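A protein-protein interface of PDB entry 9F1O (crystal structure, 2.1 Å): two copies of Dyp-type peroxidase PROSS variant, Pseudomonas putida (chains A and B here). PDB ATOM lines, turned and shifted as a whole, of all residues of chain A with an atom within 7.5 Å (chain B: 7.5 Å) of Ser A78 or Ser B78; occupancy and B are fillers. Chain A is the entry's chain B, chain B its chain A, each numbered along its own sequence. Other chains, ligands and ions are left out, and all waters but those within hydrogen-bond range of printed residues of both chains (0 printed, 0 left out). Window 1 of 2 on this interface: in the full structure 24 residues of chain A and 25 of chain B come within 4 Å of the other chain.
The side-chain carboxylate (OE1) of Glu B75 lies within hydrogen-bond range of a ring nitrogen (ND1) of His A81.
The backbone NH (N) of Ser B78 is in hydrogen-bond range of the backbone carbonyl oxygen (O) of Ser A78 (2.9 Å).
ND1 of His B81 lies within hydrogen-bond range of OE1 of Glu A75, at 2.7 Å.
The side-chain carboxylate (OE1) of Glu A75 lies close to the backbone carbonyl oxygen (O) of Gln B80, at 3.4 Å.
OE1 of Glu B75 lies close to O of Gln A80 (3.3 Å).
Among the printed residues, merely in contact across the chains: Pro A77 with Ser B78, Leu A69 with Ser B78, Ser A78 with Pro B77, Ser A78 with Leu B69, Phe A67 with Leu B69, Leu A69 with Phe B67 and Thr A79 with Thr B79.
O of Phe B67 lies within hydrogen-bond range of OG of Ser B78 (2.7 Å).
The side-chain amide nitrogen (NE2) of Gln B80 sits at hydrogen-bond distance from the backbone carbonyl oxygen (O) of Tyr B268 (2.7 Å).
The backbone carbonyl oxygen (O) of Phe A67 sits at hydrogen-bond distance from the side-chain hydroxyl (OG) of Ser A78 (2.8 Å).
N of Phe A67 lies within hydrogen-bond range of OE1 of Gln A80 (3.1 Å).
The backbone carbonyl oxygen (O) of Thr A79 lies close to a ring nitrogen (NE2) of His A81 (3.3 Å).
The side-chain amide oxygen (OE1) of Gln A80 sits at hydrogen-bond distance from the backbone NH (N) of Tyr A268, 2.7 Å away.
Ser A78 touches just these residues of chain B: Leu B69, Pro B77 and Ser B78.
Of chain A, only Leu A69, Pro A77 and Ser A78 come within 4 Å of Ser B78.
Of the printed residues of chain A, His B81 touches Glu A75 (2.7 Å).
Printed residues of chain B within 4 Å of Phe A67: Leu B69 (3.5 Å).
Of the printed residues of chain A, Leu B69 touches Phe A67 (3.5 Å) and Ser A78 (3.4 Å).
Leu A70 touches none of the printed residues of chain B.
Leu B264 touches none of the printed residues of chain A.
Of the 17 printed residues of chain B, 8 touch a printed residue of chain A.
Printed residues of chain B that touch a printed residue of chain A: Phe B67, Leu B69, Glu B75, Pro B77, Ser B78, Thr B79, Gln B80 and His B81.
Hydrophobic or aromatic side chains of chain B within 4 Å of the printed part of chain A: Leu B69, Pro B77 and His B81.
Among the printed residues, 12 pairs touch across the chains.
Leu A69 touches Ser B78, and with the chains exchanged Ser A78 touches Leu B69.
Glu A75 touches Gln B80, and with the chains exchanged Gln A80 touches Glu B75.
Pro A77 touches Ser B78, and with the chains exchanged Ser A78 touches Pro B77.
Ser A78 touches its own counterpart, Ser B78.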
ATOM      1  N   PRO A  66      20.525  20.660  -7.449  1.00  0.00           N
ATOM      2  CA  PRO A  66      20.549  20.385  -8.889  1.00  0.00           C
ATOM      3  C   PRO A  66      19.378  19.511  -9.305  1.00  0.00           C
ATOM      4  O   PRO A  66      18.777  18.795  -8.499  1.00  0.00           O
ATOM      5  CB  PRO A  66      21.883  19.656  -9.100  1.00  0.00           C
ATOM      6  CG  PRO A  66      22.692  19.946  -7.870  1.00  0.00           C
ATOM      7  CD  PRO A  66      21.697  20.082  -6.765  1.00  0.00           C
ATOM      8  N   PHE A  67      19.036  19.608 -10.585  1.00  0.00           N
ATOM      9  CA  PHE A  67      18.090  18.673 -11.171  1.00  0.00           C
ATOM     10  C   PHE A  67      18.559  17.245 -10.892  1.00  0.00           C
ATOM     11  O   PHE A  67      19.733  16.927 -11.132  1.00  0.00           O
ATOM     12  CB  PHE A  67      17.963  18.915 -12.677  1.00  0.00           C
ATOM     13  CG  PHE A  67      16.820  18.175 -13.319  1.00  0.00           C
ATOM     14  CD1 PHE A  67      16.963  16.853 -13.720  1.00  0.00           C
ATOM     15  CD2 PHE A  67      15.601  18.800 -13.519  1.00  0.00           C
ATOM     16  CE1 PHE A  67      15.909  16.173 -14.309  1.00  0.00           C
ATOM     17  CE2 PHE A  67      14.542  18.126 -14.108  1.00  0.00           C
ATOM     18  CZ  PHE A  67      14.697  16.808 -14.504  1.00  0.00           C
ATOM     19  N   PRO A  68      17.692  16.368 -10.399  1.00  0.00           N
ATOM     20  CA  PRO A  68      18.153  15.090  -9.853  1.00  0.00           C
ATOM     21  C   PRO A  68      18.501  14.085 -10.947  1.00  0.00           C
ATOM     22  O   PRO A  68      18.200  14.267 -12.127  1.00  0.00           O
ATOM     23  CB  PRO A  68      16.952  14.619  -9.028  1.00  0.00           C
ATOM     24  CG  PRO A  68      15.784  15.175  -9.773  1.00  0.00           C
ATOM     25  CD  PRO A  68      16.235  16.531 -10.258  1.00  0.00           C
ATOM     26  N   LEU A  69      19.167  13.015 -10.519  1.00  0.00           N
ATOM     27  CA  LEU A  69      19.557  11.916 -11.394  1.00  0.00           C
ATOM     28  C   LEU A  69      18.611  10.751 -11.128  1.00  0.00           C
ATOM     29  O   LEU A  69      18.680  10.115 -10.072  1.00  0.00           O
ATOM     30  CB  LEU A  69      21.010  11.514 -11.152  1.00  0.00           C
ATOM     31  CG  LEU A  69      21.538  10.345 -11.981  1.00  0.00           C
ATOM     32  CD1 LEU A  69      21.672  10.744 -13.445  1.00  0.00           C
ATOM     33  CD2 LEU A  69      22.864   9.837 -11.425  1.00  0.00           C
ATOM     34  N   LEU A  70      17.726  10.480 -12.082  1.00  0.00           N
ATOM     35  CA  LEU A  70      16.730   9.423 -11.953  1.00  0.00           C
ATOM     36  C   LEU A  70      17.241   8.179 -12.671  1.00  0.00           C
ATOM     37  O   LEU A  70      17.349   8.161 -13.902  1.00  0.00           O
ATOM     38  CB  LEU A  70      15.383   9.869 -12.517  1.00  0.00           C
ATOM     39  CG  LEU A  70      14.417  10.590 -11.570  1.00  0.00           C
ATOM     40  CD1 LEU A  70      15.053  11.814 -10.930  1.00  0.00           C
ATOM     41  CD2 LEU A  70      13.138  10.972 -12.299  1.00  0.00           C
ATOM     42  N   GLU A  75      14.674   8.229 -19.855  1.00  0.00           N
ATOM     43  CA  GLU A  75      15.789   9.163 -19.781  1.00  0.00           C
ATOM     44  C   GLU A  75      15.284  10.552 -19.412  1.00  0.00           C
ATOM     45  O   GLU A  75      14.490  11.146 -20.148  1.00  0.00           O
ATOM     46  CB  GLU A  75      16.555   9.196 -21.105  1.00  0.00           C
ATOM     47  CG  GLU A  75      17.201   7.864 -21.455  1.00  0.00           C
ATOM     48  CD  GLU A  75      17.842   7.866 -22.826  1.00  0.00           C
ATOM     49  OE1 GLU A  75      18.061   8.962 -23.378  1.00  0.00           O
ATOM     50  OE2 GLU A  75      18.124   6.768 -23.351  1.00  0.00           O
ATOM     51  N   ASN A  76      15.747  11.057 -18.270  1.00  0.00           N
ATOM     52  CA  ASN A  76      15.511  12.435 -17.846  1.00  0.00           C
ATOM     53  C   ASN A  76      16.880  13.027 -17.548  1.00  0.00           C
ATOM     54  O   ASN A  76      17.388  12.913 -16.423  1.00  0.00           O
ATOM     55  CB  ASN A  76      14.596  12.499 -16.626  1.00  0.00           C
ATOM     56  CG  ASN A  76      13.227  11.910 -16.894  1.00  0.00           C
ATOM     57  OD1 ASN A  76      12.366  12.554 -17.491  1.00  0.00           O
ATOM     58  ND2 ASN A  76      13.018  10.677 -16.446  1.00  0.00           N
ATOM     59  N   PRO A  77      17.512  13.657 -18.532  1.00  0.00           N
ATOM     60  CA  PRO A  77      18.870  14.168 -18.327  1.00  0.00           C
ATOM     61  C   PRO A  77      18.906  15.324 -17.341  1.00  0.00           C
ATOM     62  O   PRO A  77      17.931  16.058 -17.164  1.00  0.00           O
ATOM     63  CB  PRO A  77      19.290  14.625 -19.729  1.00  0.00           C
ATOM     64  CG  PRO A  77      17.993  14.927 -20.420  1.00  0.00           C
ATOM     65  CD  PRO A  77      17.023  13.910 -19.897  1.00  0.00           C
ATOM     66  N   SER A  78      20.056  15.475 -16.695  1.00  0.00           N
ATOM     67  CA  SER A  78      20.336  16.605 -15.817  1.00  0.00           C
ATOM     68  C   SER A  78      21.365  17.497 -16.503  1.00  0.00           C
ATOM     69  O   SER A  78      22.545  17.139 -16.588  1.00  0.00           O
ATOM     70  CB  SER A  78      20.834  16.130 -14.455  1.00  0.00           C
ATOM     71  OG  SER A  78      21.070  17.229 -13.592  1.00  0.00           O
ATOM     72  N   THR A  79      20.920  18.653 -16.989  1.00  0.00           N
ATOM     73  CA  THR A  79      21.824  19.622 -17.595  1.00  0.00           C
ATOM     74  C   THR A  79      21.748  20.925 -16.813  1.00  0.00           C
ATOM     75  O   THR A  79      21.325  21.960 -17.340  1.00  0.00           O
ATOM     76  CB  THR A  79      21.476  19.852 -19.068  1.00  0.00           C
ATOM     77  OG1 THR A  79      20.131  20.338 -19.173  1.00  0.00           O
ATOM     78  CG2 THR A  79      21.621  18.550 -19.865  1.00  0.00           C
ATOM     79  N   GLN A  80      22.153  20.873 -15.548  1.00  0.00           N
ATOM     80  CA  GLN A  80      22.013  22.020 -14.664  1.00  0.00           C
ATOM     81  C   GLN A  80      22.980  23.123 -15.073  1.00  0.00           C
ATOM     82  O   GLN A  80      24.165  22.871 -15.311  1.00  0.00           O
ATOM     83  CB  GLN A  80      22.261  21.602 -13.217  1.00  0.00           C
ATOM     84  CG  GLN A  80      21.964  22.692 -12.202  1.00  0.00           C
ATOM     85  CD  GLN A  80      20.512  23.124 -12.230  1.00  0.00           C
ATOM     86  OE1 GLN A  80      19.607  22.310 -12.049  1.00  0.00           O
ATOM     87  NE2 GLN A  80      20.281  24.410 -12.472  1.00  0.00           N
ATOM     88  N   HIS A  81      22.471  24.346 -15.158  1.00  0.00           N
ATOM     89  CA  HIS A  81      23.280  25.521 -15.442  1.00  0.00           C
ATOM     90  C   HIS A  81      23.225  26.484 -14.258  1.00  0.00           C
ATOM     91  O   HIS A  81      22.500  26.272 -13.283  1.00  0.00           O
ATOM     92  CB  HIS A  81      22.818  26.194 -16.737  1.00  0.00           C
ATOM     93  CG  HIS A  81      22.830  25.282 -17.924  1.00  0.00           C
ATOM     94  ND1 HIS A  81      23.983  24.693 -18.398  1.00  0.00           N
ATOM     95  CD2 HIS A  81      21.830  24.857 -18.733  1.00  0.00           C
ATOM     96  CE1 HIS A  81      23.693  23.944 -19.447  1.00  0.00           C
ATOM     97  NE2 HIS A  81      22.394  24.027 -19.672  1.00  0.00           N
ATOM     98  N   LEU A 264      15.133  16.558 -23.482  1.00  0.00           N
ATOM     99  CA  LEU A 264      16.519  16.733 -23.891  1.00  0.00           C
ATOM    100  C   LEU A 264      17.364  17.425 -22.831  1.00  0.00           C
ATOM    101  O   LEU A 264      18.589  17.253 -22.823  1.00  0.00           O
ATOM    102  CB  LEU A 264      16.586  17.539 -25.193  1.00  0.00           C
ATOM    103  CG  LEU A 264      15.698  17.056 -26.340  1.00  0.00           C
ATOM    104  CD1 LEU A 264      15.879  17.941 -27.565  1.00  0.00           C
ATOM    105  CD2 LEU A 264      15.986  15.598 -26.672  1.00  0.00           C
ATOM    106  N   THR A 265      16.741  18.191 -21.937  1.00  0.00           N
ATOM    107  CA  THR A 265      17.445  18.956 -20.918  1.00  0.00           C
ATOM    108  C   THR A 265      16.698  18.826 -19.598  1.00  0.00           C
ATOM    109  O   THR A 265      15.566  18.339 -19.542  1.00  0.00           O
ATOM    110  CB  THR A 265      17.579  20.442 -21.292  1.00  0.00           C
ATOM    111  OG1 THR A 265      16.285  21.057 -21.292  1.00  0.00           O
ATOM    112  CG2 THR A 265      18.231  20.617 -22.659  1.00  0.00           C
ATOM    113  N   GLY A 266      17.352  19.265 -18.524  1.00  0.00           N
ATOM    114  CA  GLY A 266      16.740  19.285 -17.210  1.00  0.00           C
ATOM    115  C   GLY A 266      17.416  20.252 -16.261  1.00  0.00           C
ATOM    116  O   GLY A 266      18.640  20.216 -16.104  1.00  0.00           O
ATOM    117  N   GLY A 267      16.640  21.130 -15.628  1.00  0.00           N
ATOM    118  CA  GLY A 267      17.222  22.099 -14.720  1.00  0.00           C
ATOM    119  C   GLY A 267      16.325  22.560 -13.588  1.00  0.00           C
ATOM    120  O   GLY A 267      15.112  22.712 -13.760  1.00  0.00           O
ATOM    121  N   TYR A 268      16.928  22.782 -12.423  1.00  0.00           N
ATOM    122  CA  TYR A 268      16.264  23.336 -11.250  1.00  0.00           C
ATOM    123  C   TYR A 268      16.753  24.762 -11.039  1.00  0.00           C
ATOM    124  O   TYR A 268      17.962  25.018 -11.100  1.00  0.00           O
ATOM    125  CB  TYR A 268      16.569  22.511  -9.998  1.00  0.00           C
ATOM    126  CG  TYR A 268      15.674  21.316  -9.761  1.00  0.00           C
ATOM    127  CD1 TYR A 268      14.672  20.972 -10.660  1.00  0.00           C
ATOM    128  CD2 TYR A 268      15.835  20.535  -8.627  1.00  0.00           C
ATOM    129  CE1 TYR A 268      13.856  19.872 -10.429  1.00  0.00           C
ATOM    130  CE2 TYR A 268      15.030  19.440  -8.389  1.00  0.00           C
ATOM    131  CZ  TYR A 268      14.043  19.112  -9.290  1.00  0.00           C
ATOM    132  OH  TYR A 268      13.243  18.018  -9.045  1.00  0.00           O
ATOM    133  N   PRO B  66      24.342   5.032 -13.944  1.00  0.00           N
ATOM    134  CA  PRO B  66      24.283   6.221 -14.803  1.00  0.00           C
ATOM    135  C   PRO B  66      25.457   7.151 -14.542  1.00  0.00           C
ATOM    136  O   PRO B  66      26.093   7.119 -13.485  1.00  0.00           O
ATOM    137  CB  PRO B  66      22.954   6.884 -14.418  1.00  0.00           C
ATOM    138  CG  PRO B  66      22.173   5.822 -13.708  1.00  0.00           C
ATOM    139  CD  PRO B  66      23.191   4.970 -13.026  1.00  0.00           C
ATOM    140  N   PHE B  67      25.762   7.966 -15.549  1.00  0.00           N
ATOM    141  CA  PHE B  67      26.718   9.048 -15.367  1.00  0.00           C
ATOM    142  C   PHE B  67      26.305   9.891 -14.162  1.00  0.00           C
ATOM    143  O   PHE B  67      25.139  10.299 -14.068  1.00  0.00           O
ATOM    144  CB  PHE B  67      26.801   9.912 -16.629  1.00  0.00           C
ATOM    145  CG  PHE B  67      27.939  10.899 -16.618  1.00  0.00           C
ATOM    146  CD1 PHE B  67      27.803  12.133 -16.002  1.00  0.00           C
ATOM    147  CD2 PHE B  67      29.150  10.586 -17.214  1.00  0.00           C
ATOM    148  CE1 PHE B  67      28.849  13.040 -15.987  1.00  0.00           C
ATOM    149  CE2 PHE B  67      30.202  11.488 -17.204  1.00  0.00           C
ATOM    150  CZ  PHE B  67      30.050  12.719 -16.588  1.00  0.00           C
ATOM    151  N   PRO B  68      27.215  10.177 -13.237  1.00  0.00           N
ATOM    152  CA  PRO B  68      26.814  10.713 -11.935  1.00  0.00           C
ATOM    153  C   PRO B  68      26.476  12.197 -11.996  1.00  0.00           C
ATOM    154  O   PRO B  68      26.759  12.901 -12.965  1.00  0.00           O
ATOM    155  CB  PRO B  68      28.053  10.466 -11.071  1.00  0.00           C
ATOM    156  CG  PRO B  68      29.183  10.596 -12.043  1.00  0.00           C
ATOM    157  CD  PRO B  68      28.672   9.969 -13.320  1.00  0.00           C
ATOM    158  N   LEU B  69      25.853  12.658 -10.917  1.00  0.00           N
ATOM    159  CA  LEU B  69      25.482  14.055 -10.736  1.00  0.00           C
ATOM    160  C   LEU B  69      26.457  14.685  -9.750  1.00  0.00           C
ATOM    161  O   LEU B  69      26.420  14.382  -8.553  1.00  0.00           O
ATOM    162  CB  LEU B  69      24.043  14.167 -10.235  1.00  0.00           C
ATOM    163  CG  LEU B  69      23.519  15.573  -9.942  1.00  0.00           C
ATOM    164  CD1 LEU B  69      23.348  16.373 -11.225  1.00  0.00           C
ATOM    165  CD2 LEU B  69      22.212  15.499  -9.165  1.00  0.00           C
ATOM    166  N   LEU B  70      27.331  15.554 -10.252  1.00  0.00           N
ATOM    167  CA  LEU B  70      28.335  16.220  -9.429  1.00  0.00           C
ATOM    168  C   LEU B  70      27.809  17.600  -9.053  1.00  0.00           C
ATOM    169  O   LEU B  70      27.682  18.480  -9.911  1.00  0.00           O
ATOM    170  CB  LEU B  70      29.674  16.317 -10.160  1.00  0.00           C
ATOM    171  CG  LEU B  70      30.654  15.145 -10.021  1.00  0.00           C
ATOM    172  CD1 LEU B  70      30.030  13.822 -10.444  1.00  0.00           C
ATOM    173  CD2 LEU B  70      31.930  15.415 -10.804  1.00  0.00           C
ATOM    174  N   GLU B  75      29.997  22.528 -14.298  1.00  0.00           N
ATOM    175  CA  GLU B  75      28.876  21.781 -14.851  1.00  0.00           C
ATOM    176  C   GLU B  75      29.385  20.554 -15.596  1.00  0.00           C
ATOM    177  O   GLU B  75      30.137  20.679 -16.569  1.00  0.00           O
ATOM    178  CB  GLU B  75      28.045  22.671 -15.774  1.00  0.00           C
ATOM    179  CG  GLU B  75      27.415  23.856 -15.061  1.00  0.00           C
ATOM    180  CD  GLU B  75      26.710  24.802 -16.011  1.00  0.00           C
ATOM    181  OE1 GLU B  75      26.433  24.400 -17.161  1.00  0.00           O
ATOM    182  OE2 GLU B  75      26.445  25.956 -15.612  1.00  0.00           O
ATOM    183  N   ASN B  76      28.971  19.375 -15.137  1.00  0.00           N
ATOM    184  CA  ASN B  76      29.202  18.111 -15.836  1.00  0.00           C
ATOM    185  C   ASN B  76      27.835  17.470 -16.010  1.00  0.00           C
ATOM    186  O   ASN B  76      27.357  16.752 -15.121  1.00  0.00           O
ATOM    187  CB  ASN B  76      30.154  17.194 -15.069  1.00  0.00           C
ATOM    188  CG  ASN B  76      31.533  17.793 -14.896  1.00  0.00           C
ATOM    189  OD1 ASN B  76      32.354  17.769 -15.813  1.00  0.00           O
ATOM    190  ND2 ASN B  76      31.804  18.321 -13.708  1.00  0.00           N
ATOM    191  N   PRO B  77      27.173  17.710 -17.137  1.00  0.00           N
ATOM    192  CA  PRO B  77      25.812  17.197 -17.313  1.00  0.00           C
ATOM    193  C   PRO B  77      25.785  15.680 -17.392  1.00  0.00           C
ATOM    194  O   PRO B  77      26.752  15.032 -17.801  1.00  0.00           O
ATOM    195  CB  PRO B  77      25.365  17.827 -18.637  1.00  0.00           C
ATOM    196  CG  PRO B  77      26.642  18.088 -19.370  1.00  0.00           C
ATOM    197  CD  PRO B  77      27.634  18.471 -18.312  1.00  0.00           C
ATOM    198  N   SER B  78      24.651  15.116 -16.988  1.00  0.00           N
ATOM    199  CA  SER B  78      24.383  13.689 -17.113  1.00  0.00           C
ATOM    200  C   SER B  78      23.327  13.509 -18.195  1.00  0.00           C
ATOM    201  O   SER B  78      22.148  13.804 -17.974  1.00  0.00           O
ATOM    202  CB  SER B  78      23.922  13.098 -15.782  1.00  0.00           C
ATOM    203  OG  SER B  78      23.704  11.704 -15.893  1.00  0.00           O
ATOM    204  N   THR B  79      23.750  13.019 -19.358  1.00  0.00           N
ATOM    205  CA  THR B  79      22.832  12.738 -20.454  1.00  0.00           C
ATOM    206  C   THR B  79      22.908  11.260 -20.814  1.00  0.00           C
ATOM    207  O   THR B  79      23.321  10.895 -21.920  1.00  0.00           O
ATOM    208  CB  THR B  79      23.154  13.615 -21.666  1.00  0.00           C
ATOM    209  OG1 THR B  79      24.503  13.378 -22.086  1.00  0.00           O
ATOM    210  CG2 THR B  79      22.994  15.088 -21.317  1.00  0.00           C
ATOM    211  N   GLN B  80      22.515  10.408 -19.870  1.00  0.00           N
ATOM    212  CA  GLN B  80      22.655   8.969 -20.036  1.00  0.00           C
ATOM    213  C   GLN B  80      21.669   8.439 -21.071  1.00  0.00           C
ATOM    214  O   GLN B  80      20.483   8.782 -21.048  1.00  0.00           O
ATOM    215  CB  GLN B  80      22.440   8.265 -18.698  1.00  0.00           C
ATOM    216  CG  GLN B  80      22.759   6.785 -18.736  1.00  0.00           C
ATOM    217  CD  GLN B  80      24.211   6.534 -19.082  1.00  0.00           C
ATOM    218  OE1 GLN B  80      25.113   7.022 -18.401  1.00  0.00           O
ATOM    219  NE2 GLN B  80      24.446   5.784 -20.153  1.00  0.00           N
ATOM    220  N   HIS B  81      22.162   7.606 -21.980  1.00  0.00           N
ATOM    221  CA  HIS B  81      21.332   6.923 -22.962  1.00  0.00           C
ATOM    222  C   HIS B  81      21.426   5.410 -22.772  1.00  0.00           C
ATOM    223  O   HIS B  81      22.196   4.903 -21.952  1.00  0.00           O
ATOM    224  CB  HIS B  81      21.719   7.336 -24.385  1.00  0.00           C
ATOM    225  CG  HIS B  81      21.634   8.811 -24.623  1.00  0.00           C
ATOM    226  ND1 HIS B  81      20.452   9.511 -24.523  1.00  0.00           N
ATOM    227  CD2 HIS B  81      22.583   9.719 -24.950  1.00  0.00           C
ATOM    228  CE1 HIS B  81      20.674  10.788 -24.778  1.00  0.00           C
ATOM    229  NE2 HIS B  81      21.959  10.941 -25.042  1.00  0.00           N
ATOM    230  N   LEU B 264      29.337  19.116 -22.837  1.00  0.00           N
ATOM    231  CA  LEU B 264      27.933  19.249 -23.200  1.00  0.00           C
ATOM    232  C   LEU B 264      27.126  17.994 -22.899  1.00  0.00           C
ATOM    233  O   LEU B 264      25.905  18.084 -22.734  1.00  0.00           O
ATOM    234  CB  LEU B 264      27.798  19.588 -24.688  1.00  0.00           C
ATOM    235  CG  LEU B 264      28.635  20.766 -25.187  1.00  0.00           C
ATOM    236  CD1 LEU B 264      28.392  20.994 -26.670  1.00  0.00           C
ATOM    237  CD2 LEU B 264      28.333  22.028 -24.387  1.00  0.00           C
ATOM    238  N   THR B 265      27.780  16.836 -22.814  1.00  0.00           N
ATOM    239  CA  THR B 265      27.105  15.565 -22.595  1.00  0.00           C
ATOM    240  C   THR B 265      27.888  14.756 -21.571  1.00  0.00           C
ATOM    241  O   THR B 265      29.035  15.067 -21.241  1.00  0.00           O
ATOM    242  CB  THR B 265      26.966  14.756 -23.896  1.00  0.00           C
ATOM    243  OG1 THR B 265      28.263  14.340 -24.344  1.00  0.00           O
ATOM    244  CG2 THR B 265      26.291  15.575 -24.989  1.00  0.00           C
ATOM    245  N   GLY B 266      27.251  13.701 -21.068  1.00  0.00           N
ATOM    246  CA  GLY B 266      27.897  12.787 -20.145  1.00  0.00           C
ATOM    247  C   GLY B 266      27.205  11.440 -20.093  1.00  0.00           C
ATOM    248  O   GLY B 266      25.991  11.373 -19.879  1.00  0.00           O
ATOM    249  N   GLY B 267      27.960  10.360 -20.283  1.00  0.00           N
ATOM    250  CA  GLY B 267      27.370   9.037 -20.271  1.00  0.00           C
ATOM    251  C   GLY B 267      28.294   7.923 -19.822  1.00  0.00           C
ATOM    252  O   GLY B 267      29.490   7.926 -20.129  1.00  0.00           O
ATOM    253  N   TYR B 268      27.733   6.956 -19.102  1.00  0.00           N
ATOM    254  CA  TYR B 268      28.434   5.755 -18.667  1.00  0.00           C
ATOM    255  C   TYR B 268      27.925   4.577 -19.482  1.00  0.00           C
ATOM    256  O   TYR B 268      26.713   4.430 -19.665  1.00  0.00           O
ATOM    257  CB  TYR B 268      28.193   5.480 -17.182  1.00  0.00           C
ATOM    258  CG  TYR B 268      29.101   6.209 -16.220  1.00  0.00           C
ATOM    259  CD1 TYR B 268      30.060   7.111 -16.665  1.00  0.00           C
ATOM    260  CD2 TYR B 268      28.997   5.986 -14.855  1.00  0.00           C
ATOM    261  CE1 TYR B 268      30.888   7.775 -15.766  1.00  0.00           C
ATOM    262  CE2 TYR B 268      29.815   6.639 -13.956  1.00  0.00           C
ATOM    263  CZ  TYR B 268      30.759   7.530 -14.411  1.00  0.00           C
ATOM    264  OH  TYR B 268      31.565   8.175 -13.497  1.00  0.00           O
